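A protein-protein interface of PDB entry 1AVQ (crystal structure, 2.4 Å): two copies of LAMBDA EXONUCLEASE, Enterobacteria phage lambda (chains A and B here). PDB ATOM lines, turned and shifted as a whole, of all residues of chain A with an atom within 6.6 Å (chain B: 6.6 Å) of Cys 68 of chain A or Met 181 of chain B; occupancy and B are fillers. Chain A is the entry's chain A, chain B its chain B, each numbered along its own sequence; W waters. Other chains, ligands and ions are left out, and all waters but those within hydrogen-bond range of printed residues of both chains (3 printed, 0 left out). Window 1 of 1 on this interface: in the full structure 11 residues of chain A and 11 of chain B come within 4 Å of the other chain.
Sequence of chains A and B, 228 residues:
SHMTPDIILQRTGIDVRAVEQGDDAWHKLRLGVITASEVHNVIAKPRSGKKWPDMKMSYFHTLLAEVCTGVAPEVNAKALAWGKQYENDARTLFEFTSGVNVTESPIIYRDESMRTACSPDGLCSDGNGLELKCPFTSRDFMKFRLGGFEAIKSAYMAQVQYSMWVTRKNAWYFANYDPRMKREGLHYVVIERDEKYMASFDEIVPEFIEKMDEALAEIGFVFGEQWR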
ATOM      1  N   LEU A  63       9.596  21.794  26.369  1.00  0.00           N
ATOM      2  CA  LEU A  63       9.532  20.577  27.213  1.00  0.00           C
ATOM      3  C   LEU A  63       8.309  20.660  28.138  1.00  0.00           C
ATOM      4  O   LEU A  63       7.578  19.700  28.315  1.00  0.00           O
ATOM      5  CB  LEU A  63      10.866  20.341  28.012  1.00  0.00           C
ATOM      6  CG  LEU A  63      11.635  19.040  27.779  1.00  0.00           C
ATOM      7  CD1 LEU A  63      11.496  18.541  26.343  1.00  0.00           C
ATOM      8  CD2 LEU A  63      13.111  19.129  28.204  1.00  0.00           C
ATOM      9  N   LEU A  64       8.111  21.839  28.721  1.00  0.00           N
ATOM     10  CA  LEU A  64       7.029  22.063  29.649  1.00  0.00           C
ATOM     11  C   LEU A  64       5.725  21.875  28.949  1.00  0.00           C
ATOM     12  O   LEU A  64       4.811  21.230  29.446  1.00  0.00           O
ATOM     13  CB  LEU A  64       7.045  23.493  30.257  1.00  0.00           C
ATOM     14  CG  LEU A  64       8.205  23.709  31.215  1.00  0.00           C
ATOM     15  CD1 LEU A  64       8.380  25.196  31.478  1.00  0.00           C
ATOM     16  CD2 LEU A  64       8.075  22.919  32.518  1.00  0.00           C
ATOM     17  N   ALA A  65       5.646  22.479  27.817  1.00  0.00           N
ATOM     18  CA  ALA A  65       4.432  22.368  27.132  1.00  0.00           C
ATOM     19  C   ALA A  65       4.106  20.926  26.755  1.00  0.00           C
ATOM     20  O   ALA A  65       2.926  20.534  26.615  1.00  0.00           O
ATOM     21  CB  ALA A  65       4.553  23.266  25.915  1.00  0.00           C
ATOM     22  N   GLU A  66       5.141  20.111  26.526  1.00  0.00           N
ATOM     23  CA  GLU A  66       4.842  18.691  26.204  1.00  0.00           C
ATOM     24  C   GLU A  66       4.161  17.970  27.417  1.00  0.00           C
ATOM     25  O   GLU A  66       3.292  17.089  27.274  1.00  0.00           O
ATOM     26  CB  GLU A  66       6.120  17.902  25.828  1.00  0.00           C
ATOM     27  CG  GLU A  66       6.722  18.248  24.448  1.00  0.00           C
ATOM     28  CD  GLU A  66       8.025  17.531  24.115  1.00  0.00           C
ATOM     29  OE1 GLU A  66       8.683  16.844  24.921  1.00  0.00           O
ATOM     30  OE2 GLU A  66       8.392  17.737  22.852  1.00  0.00           O
ATOM     31  N   VAL A  67       4.608  18.359  28.625  1.00  0.00           N
ATOM     32  CA  VAL A  67       4.078  17.881  29.858  1.00  0.00           C
ATOM     33  C   VAL A  67       2.607  18.264  30.020  1.00  0.00           C
ATOM     34  O   VAL A  67       1.724  17.430  30.307  1.00  0.00           O
ATOM     35  CB  VAL A  67       4.904  18.232  31.095  1.00  0.00           C
ATOM     36  CG1 VAL A  67       4.320  17.584  32.374  1.00  0.00           C
ATOM     37  CG2 VAL A  67       6.350  17.765  30.944  1.00  0.00           C
ATOM     38  N   CYS A  68       2.320  19.512  29.844  1.00  0.00           N
ATOM     39  CA  CYS A  68       0.923  19.972  30.038  1.00  0.00           C
ATOM     40  C   CYS A  68      -0.060  19.751  28.890  1.00  0.00           C
ATOM     41  O   CYS A  68      -1.242  19.974  29.076  1.00  0.00           O
ATOM     42  CB  CYS A  68       0.875  21.434  30.492  1.00  0.00           C
ATOM     43  SG  CYS A  68       2.194  21.815  31.690  1.00  0.00           S
ATOM     44  N   THR A  69       0.399  19.359  27.684  1.00  0.00           N
ATOM     45  CA  THR A  69      -0.516  19.073  26.587  1.00  0.00           C
ATOM     46  C   THR A  69      -0.444  17.583  26.351  1.00  0.00           C
ATOM     47  O   THR A  69      -1.374  16.988  25.840  1.00  0.00           O
ATOM     48  CB  THR A  69      -0.095  19.700  25.245  1.00  0.00           C
ATOM     49  OG1 THR A  69       1.152  19.149  24.839  1.00  0.00           O
ATOM     50  CG2 THR A  69       0.045  21.205  25.377  1.00  0.00           C
ATOM     51  N   GLY A  70       0.702  16.939  26.613  1.00  0.00           N
ATOM     52  CA  GLY A  70       0.740  15.516  26.260  1.00  0.00           C
ATOM     53  C   GLY A  70       0.882  15.264  24.723  1.00  0.00           C
ATOM     54  O   GLY A  70       0.630  14.159  24.218  1.00  0.00           O
ATOM     55  N   VAL A  71       1.260  16.290  23.936  1.00  0.00           N
ATOM     56  CA  VAL A  71       1.530  16.083  22.512  1.00  0.00           C
ATOM     57  C   VAL A  71       2.798  16.883  22.166  1.00  0.00           C
ATOM     58  O   VAL A  71       3.301  17.712  22.982  1.00  0.00           O
ATOM     59  CB  VAL A  71       0.407  16.509  21.520  1.00  0.00           C
ATOM     60  CG1 VAL A  71      -0.815  15.702  21.774  1.00  0.00           C
ATOM     61  CG2 VAL A  71       0.019  17.955  21.706  1.00  0.00           C
ATOM     62  N   LEU A 216       6.331  23.915  36.651  1.00  0.00           N
ATOM     63  CA  LEU A 216       5.103  23.105  36.528  1.00  0.00           C
ATOM     64  C   LEU A 216       4.210  23.229  37.758  1.00  0.00           C
ATOM     65  O   LEU A 216       2.973  23.194  37.687  1.00  0.00           O
ATOM     66  CB  LEU A 216       5.422  21.583  36.438  1.00  0.00           C
ATOM     67  CG  LEU A 216       6.123  21.149  35.141  1.00  0.00           C
ATOM     68  CD1 LEU A 216       6.784  19.806  35.358  1.00  0.00           C
ATOM     69  CD2 LEU A 216       5.158  21.058  33.945  1.00  0.00           C
ATOM     70  N   ILE A 219       1.981  26.095  37.929  1.00  0.00           N
ATOM     71  CA  ILE A 219       0.723  26.173  37.150  1.00  0.00           C
ATOM     72  C   ILE A 219      -0.126  24.967  37.408  1.00  0.00           C
ATOM     73  O   ILE A 219      -1.031  24.644  36.651  1.00  0.00           O
ATOM     74  CB  ILE A 219       0.934  26.404  35.676  1.00  0.00           C
ATOM     75  CG1 ILE A 219       1.658  25.220  35.066  1.00  0.00           C
ATOM     76  CG2 ILE A 219       1.771  27.657  35.439  1.00  0.00           C
ATOM     77  CD1 ILE A 219       1.998  25.436  33.572  1.00  0.00           C
ATOM     78  N   PHE A 221       0.873  21.611  37.635  1.00  0.00           N
ATOM     79  CA  PHE A 221       0.944  20.341  36.949  1.00  0.00           C
ATOM     80  C   PHE A 221       2.063  19.610  37.632  1.00  0.00           C
ATOM     81  O   PHE A 221       2.920  20.236  38.286  1.00  0.00           O
ATOM     82  CB  PHE A 221       1.423  20.628  35.505  1.00  0.00           C
ATOM     83  CG  PHE A 221       0.295  20.738  34.544  1.00  0.00           C
ATOM     84  CD1 PHE A 221      -0.331  21.971  34.334  1.00  0.00           C
ATOM     85  CD2 PHE A 221      -0.160  19.606  33.855  1.00  0.00           C
ATOM     86  CE1 PHE A 221      -1.443  22.095  33.484  1.00  0.00           C
ATOM     87  CE2 PHE A 221      -1.245  19.734  32.972  1.00  0.00           C
ATOM     88  CZ  PHE A 221      -1.904  20.966  32.791  1.00  0.00           C
ATOM     89  N   GLU A 225       2.312  13.867  33.953  1.00  0.00           N
ATOM     90  CA  GLU A 225       0.907  13.904  33.511  1.00  0.00           C
ATOM     91  C   GLU A 225       0.739  13.494  32.034  1.00  0.00           C
ATOM     92  O   GLU A 225      -0.356  13.117  31.536  1.00  0.00           O
ATOM     93  CB  GLU A 225       0.158  15.220  33.888  1.00  0.00           C
ATOM     94  CG  GLU A 225       0.256  15.636  35.383  1.00  0.00           C
ATOM     95  CD  GLU A 225      -0.763  16.685  35.788  1.00  0.00           C
ATOM     96  OE1 GLU A 225      -1.903  16.465  35.179  1.00  0.00           O
ATOM     97  OE2 GLU A 225      -0.536  17.656  36.524  1.00  0.00           O
ATOM     98  N   GLN A 226       1.872  13.569  31.327  1.00  0.00           N
ATOM     99  CA  GLN A 226       1.885  13.266  29.905  1.00  0.00           C
ATOM    100  C   GLN A 226       1.653  11.816  29.633  1.00  0.00           C
ATOM    101  O   GLN A 226       1.342  11.493  28.514  1.00  0.00           O
ATOM    102  CB  GLN A 226       3.165  13.741  29.181  1.00  0.00           C
ATOM    103  CG  GLN A 226       4.507  13.067  29.649  1.00  0.00           C
ATOM    104  CD  GLN A 226       5.165  13.665  30.888  1.00  0.00           C
ATOM    105  OE1 GLN A 226       6.378  13.522  31.049  1.00  0.00           O
ATOM    106  NE2 GLN A 226       4.379  14.250  31.822  1.00  0.00           N
ATOM    107  N   SER B 138       2.626  25.616  21.188  1.00  0.00           N
ATOM    108  CA  SER B 138       2.326  25.588  22.615  1.00  0.00           C
ATOM    109  C   SER B 138       3.466  26.232  23.416  1.00  0.00           C
ATOM    110  O   SER B 138       3.272  26.893  24.431  1.00  0.00           O
ATOM    111  CB  SER B 138       1.928  24.195  23.114  1.00  0.00           C
ATOM    112  OG  SER B 138       0.751  23.707  22.467  1.00  0.00           O
ATOM    113  N   PHE B 141       2.812  29.840  23.880  1.00  0.00           N
ATOM    114  CA  PHE B 141       1.791  29.918  24.882  1.00  0.00           C
ATOM    115  C   PHE B 141       2.438  29.844  26.294  1.00  0.00           C
ATOM    116  O   PHE B 141       2.204  30.718  27.143  1.00  0.00           O
ATOM    117  CB  PHE B 141       0.698  28.848  24.726  1.00  0.00           C
ATOM    118  CG  PHE B 141      -0.246  28.958  25.892  1.00  0.00           C
ATOM    119  CD1 PHE B 141      -1.348  29.824  25.854  1.00  0.00           C
ATOM    120  CD2 PHE B 141      -0.054  28.208  27.064  1.00  0.00           C
ATOM    121  CE1 PHE B 141      -2.248  29.922  26.926  1.00  0.00           C
ATOM    122  CE2 PHE B 141      -0.927  28.301  28.164  1.00  0.00           C
ATOM    123  CZ  PHE B 141      -2.025  29.169  28.092  1.00  0.00           C
ATOM    124  N   MET B 142       3.295  28.834  26.521  1.00  0.00           N
ATOM    125  CA  MET B 142       3.963  28.654  27.802  1.00  0.00           C
ATOM    126  C   MET B 142       4.780  29.844  28.157  1.00  0.00           C
ATOM    127  O   MET B 142       4.862  30.230  29.318  1.00  0.00           O
ATOM    128  CB  MET B 142       4.896  27.415  27.973  1.00  0.00           C
ATOM    129  CG  MET B 142       4.183  26.138  28.401  1.00  0.00           C
ATOM    130  SD  MET B 142       3.915  25.976  30.196  1.00  0.00           S
ATOM    131  CE  MET B 142       5.043  27.316  30.549  1.00  0.00           C
ATOM    132  N   ARG B 145       2.383  32.470  29.463  1.00  0.00           N
ATOM    133  CA  ARG B 145       1.715  31.958  30.614  1.00  0.00           C
ATOM    134  C   ARG B 145       2.548  32.094  31.842  1.00  0.00           C
ATOM    135  O   ARG B 145       2.042  32.363  32.931  1.00  0.00           O
ATOM    136  CB  ARG B 145       1.462  30.502  30.473  1.00  0.00           C
ATOM    137  CG  ARG B 145       1.039  29.907  31.806  1.00  0.00           C
ATOM    138  CD  ARG B 145      -0.321  30.500  32.072  1.00  0.00           C
ATOM    139  NE  ARG B 145      -1.038  29.939  33.190  1.00  0.00           N
ATOM    140  CZ  ARG B 145      -0.711  30.271  34.433  1.00  0.00           C
ATOM    141  NH1 ARG B 145       0.266  31.128  34.682  1.00  0.00           N
ATOM    142  NH2 ARG B 145      -1.390  29.778  35.456  1.00  0.00           N
ATOM    143  N   ASP B 178      -4.851  28.350  24.241  1.00  0.00           N
ATOM    144  CA  ASP B 178      -4.281  27.188  23.617  1.00  0.00           C
ATOM    145  C   ASP B 178      -5.138  26.027  23.878  1.00  0.00           C
ATOM    146  O   ASP B 178      -5.175  25.491  24.984  1.00  0.00           O
ATOM    147  CB  ASP B 178      -2.860  26.862  24.059  1.00  0.00           C
ATOM    148  CG  ASP B 178      -2.298  25.647  23.346  1.00  0.00           C
ATOM    149  OD1 ASP B 178      -2.947  24.889  22.607  1.00  0.00           O
ATOM    150  OD2 ASP B 178      -1.035  25.525  23.587  1.00  0.00           O
ATOM    151  N   PRO B 179      -5.842  25.639  22.868  1.00  0.00           N
ATOM    152  CA  PRO B 179      -6.747  24.511  23.049  1.00  0.00           C
ATOM    153  C   PRO B 179      -5.999  23.238  23.429  1.00  0.00           C
ATOM    154  O   PRO B 179      -6.613  22.222  23.768  1.00  0.00           O
ATOM    155  CB  PRO B 179      -7.438  24.275  21.698  1.00  0.00           C
ATOM    156  CG  PRO B 179      -6.539  24.998  20.679  1.00  0.00           C
ATOM    157  CD  PRO B 179      -5.609  25.964  21.449  1.00  0.00           C
ATOM    158  N   ARG B 180      -4.665  23.257  23.309  1.00  0.00           N
ATOM    159  CA  ARG B 180      -3.898  22.043  23.571  1.00  0.00           C
ATOM    160  C   ARG B 180      -3.613  21.763  25.024  1.00  0.00           C
ATOM    161  O   ARG B 180      -3.400  20.594  25.431  1.00  0.00           O
ATOM    162  CB  ARG B 180      -2.687  21.841  22.672  1.00  0.00           C
ATOM    163  CG  ARG B 180      -3.038  21.529  21.181  1.00  0.00           C
ATOM    164  CD  ARG B 180      -1.954  22.115  20.287  1.00  0.00           C
ATOM    165  NE  ARG B 180      -1.809  23.545  20.576  1.00  0.00           N
ATOM    166  CZ  ARG B 180      -1.167  24.447  19.809  1.00  0.00           C
ATOM    167  NH1 ARG B 180      -0.513  24.088  18.739  1.00  0.00           N
ATOM    168  NH2 ARG B 180      -1.122  25.744  20.132  1.00  0.00           N
ATOM    169  N   MET B 181      -3.601  22.836  25.803  1.00  0.00           N
ATOM    170  CA  MET B 181      -3.349  22.705  27.214  1.00  0.00           C
ATOM    171  C   MET B 181      -4.403  21.848  27.844  1.00  0.00           C
ATOM    172  O   MET B 181      -5.562  22.026  27.560  1.00  0.00           O
ATOM    173  CB  MET B 181      -3.330  24.081  27.832  1.00  0.00           C
ATOM    174  CG  MET B 181      -2.082  24.753  27.353  1.00  0.00           C
ATOM    175  SD  MET B 181      -0.555  24.040  28.083  1.00  0.00           S
ATOM    176  CE  MET B 181      -0.710  24.556  29.838  1.00  0.00           C
ATOM    177  N   LYS B 182      -4.023  20.845  28.609  1.00  0.00           N
ATOM    178  CA  LYS B 182      -5.045  20.000  29.215  1.00  0.00           C
ATOM    179  C   LYS B 182      -5.897  20.813  30.231  1.00  0.00           C
ATOM    180  O   LYS B 182      -7.078  20.549  30.417  1.00  0.00           O
ATOM    181  CB  LYS B 182      -4.436  18.767  29.873  1.00  0.00           C
ATOM    182  CG  LYS B 182      -3.719  17.906  28.882  1.00  0.00           C
ATOM    183  CD  LYS B 182      -4.713  17.044  28.132  1.00  0.00           C
ATOM    184  CE  LYS B 182      -4.340  15.573  28.195  1.00  0.00           C
ATOM    185  NZ  LYS B 182      -4.107  14.974  26.861  1.00  0.00           N
ATOM    186  N   ARG B 183      -5.247  21.797  30.870  1.00  0.00           N
ATOM    187  CA  ARG B 183      -5.794  22.711  31.827  1.00  0.00           C
ATOM    188  C   ARG B 183      -5.065  24.000  31.571  1.00  0.00           C
ATOM    189  O   ARG B 183      -4.041  23.975  30.898  1.00  0.00           O
ATOM    190  CB  ARG B 183      -5.415  22.283  33.273  1.00  0.00           C
ATOM    191  CG  ARG B 183      -6.129  21.030  33.717  1.00  0.00           C
ATOM    192  CD  ARG B 183      -5.912  20.604  35.168  1.00  0.00           C
ATOM    193  NE  ARG B 183      -4.529  20.574  35.707  1.00  0.00           N
ATOM    194  CZ  ARG B 183      -3.766  19.475  35.829  1.00  0.00           C
ATOM    195  NH1 ARG B 183      -4.119  18.276  35.354  1.00  0.00           N
ATOM    196  NH2 ARG B 183      -2.594  19.596  36.427  1.00  0.00           N
ATOM    197  N   GLU B 184      -5.544  25.094  32.156  1.00  0.00           N
ATOM    198  CA  GLU B 184      -4.881  26.401  32.089  1.00  0.00           C
ATOM    199  C   GLU B 184      -4.531  26.936  30.711  1.00  0.00           C
ATOM    200  O   GLU B 184      -3.505  27.616  30.548  1.00  0.00           O
ATOM    201  CB  GLU B 184      -3.604  26.310  32.923  1.00  0.00           C
ATOM    202  CG  GLU B 184      -3.937  25.791  34.331  1.00  0.00           C
ATOM    203  CD  GLU B 184      -3.699  26.844  35.377  1.00  0.00           C
ATOM    204  OE1 GLU B 184      -2.672  27.589  35.098  1.00  0.00           O
ATOM    205  OE2 GLU B 184      -4.407  27.033  36.346  1.00  0.00           O
ATOM    206  N   GLY B 185      -5.374  26.651  29.731  1.00  0.00           N
ATOM    207  CA  GLY B 185      -5.142  27.093  28.336  1.00  0.00           C
ATOM    208  C   GLY B 185      -5.537  28.541  27.964  1.00  0.00           C
ATOM    209  O   GLY B 185      -5.590  28.856  26.793  1.00  0.00           O
ATOM    210  N   LEU B 186      -5.757  29.400  28.963  1.00  0.00           N
ATOM    211  CA  LEU B 186      -6.101  30.811  28.827  1.00  0.00           C
ATOM    212  C   LEU B 186      -5.340  31.693  29.768  1.00  0.00           C
ATOM    213  O   LEU B 186      -5.314  31.455  30.923  1.00  0.00           O
ATOM    214  CB  LEU B 186      -7.572  31.129  29.085  1.00  0.00           C
ATOM    215  CG  LEU B 186      -7.986  32.552  28.632  1.00  0.00           C
ATOM    216  CD1 LEU B 186      -8.605  32.517  27.228  1.00  0.00           C
ATOM    217  CD2 LEU B 186      -9.007  33.115  29.608  1.00  0.00           C
HETATM  218  O   HOH W   1      -3.849  18.082  24.280  1.00  0.00           O
HETATM  219  O   HOH W   2      -3.599  22.916  36.600  1.00  0.00           O
HETATM  220  O   HOH W   3      -1.775  13.994  28.501  1.00  0.00           O
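Of the 13 printed residues of chain B, 8 touch a printed residue of chain A.
Hydrophobic or aromatic side chains of chain B within 4 Å of the printed part of chain A: Met 142 and Met 181.
Along chain B the printed residues that touch a printed residue of chain A span positions 138 to 184.
Of the 14 printed residues of chain A, 7 touch a printed residue of chain B.
Printed residues of chain A that touch a printed residue of chain B: Leu 64, Ala 65, Cys 68, Thr 69, Ile 219, Phe 221 and Glu 225.
Hydrophobic or aromatic side chains of chain A within 4 Å of the printed part of chain B: Leu 64, Ala 65, Ile 219 and Phe 221.
Among the printed residues, 14 pairs touch across the chains.
Water W2 bridges NE of Arg 183 of chain B and O of Ile 219 of chain A.
Water W1 bridges the backbone carbonyl oxygen of Arg 180 of chain B (2.8 Å) and the backbone carbonyl oxygen of Thr 69 of chain A (3.1 Å).
Water W3 lies within hydrogen-bond range of the side-chain amino group of Lys 182 of chain B and the backbone carbonyl oxygen of Glu 225 of chain A.
OG of Ser 138 of chain B is in hydrogen-bond range of OD2 of Asp 178 of chain B (2.8 Å).
OG of Ser 138 of chain B lies within hydrogen-bond range of NE of Arg 180 of chain B, 3.2 Å away.
OG1 of Thr 69 of chain A lies within hydrogen-bond range of O of Ala 65 of chain A (2.9 Å).
N of Phe 221 of chain A lies within hydrogen-bond range of O of Leu 216 of chain A (2.6 Å).
OG1 of Thr 69 of chain A lies within hydrogen-bond range of N of Val 71 of chain A (3.0 Å).
SG of Cys 68 of chain A is in hydrogen-bond range of O of Leu 64 of chain A, 3.5 Å away.
Met 142 of chain B touches Leu 64 of chain A (SD to CB, 3.996 Å).
Met 142 of chain B touches Ala 65 of chain A (CG to CB, 3.8 Å).
Thr 69 of chain A touches Ser 138 of chain B (CG2 to OG, 3.9 Å).
CB of Thr 69 of chain A touches O of Arg 180 of chain B, 3.4 Å away.
Met 181 of chain B touches Thr 69 of chain A.
Thr 69 of chain A touches Lys 182 of chain B.
SD of Met 142 of chain B touches CD1 of Ile 219 of chain A, at 3.9 Å.
Arg 145 of chain B touches Ile 219 of chain A (CZ to CG2, 3.7 Å).
Ile 219 of chain A touches Glu 184 of chain B (O to CD, 3.7 Å).
Arg 183 of chain B touches Phe 221 of chain A (NH2 to CD2, 3.5 Å).
The guanidinium group of Arg 183 of chain B is in salt-bridge range of the side-chain carboxylate of Glu 225 of chain A, 2.8 Å away.
The backbone NH (N) of Lys 182 of chain B lies within hydrogen-bond range of the backbone carbonyl oxygen (O) of Cys 68 of chain A (3.0 Å).
Printed residues of chain A within 4 Å of Arg 183 of chain B: Phe 221 and Glu 225.
Of the printed residues of chain A, Arg 145 of chain B touches Ile 219.
Of the printed residues of chain B, Ala 65 of chain A touches Ser 138 and Met 142.
No position is printed for both chains.
Of the 14 pairs that touch across the chains among the printed residues, none has its exchanged pair printed and touching as well.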
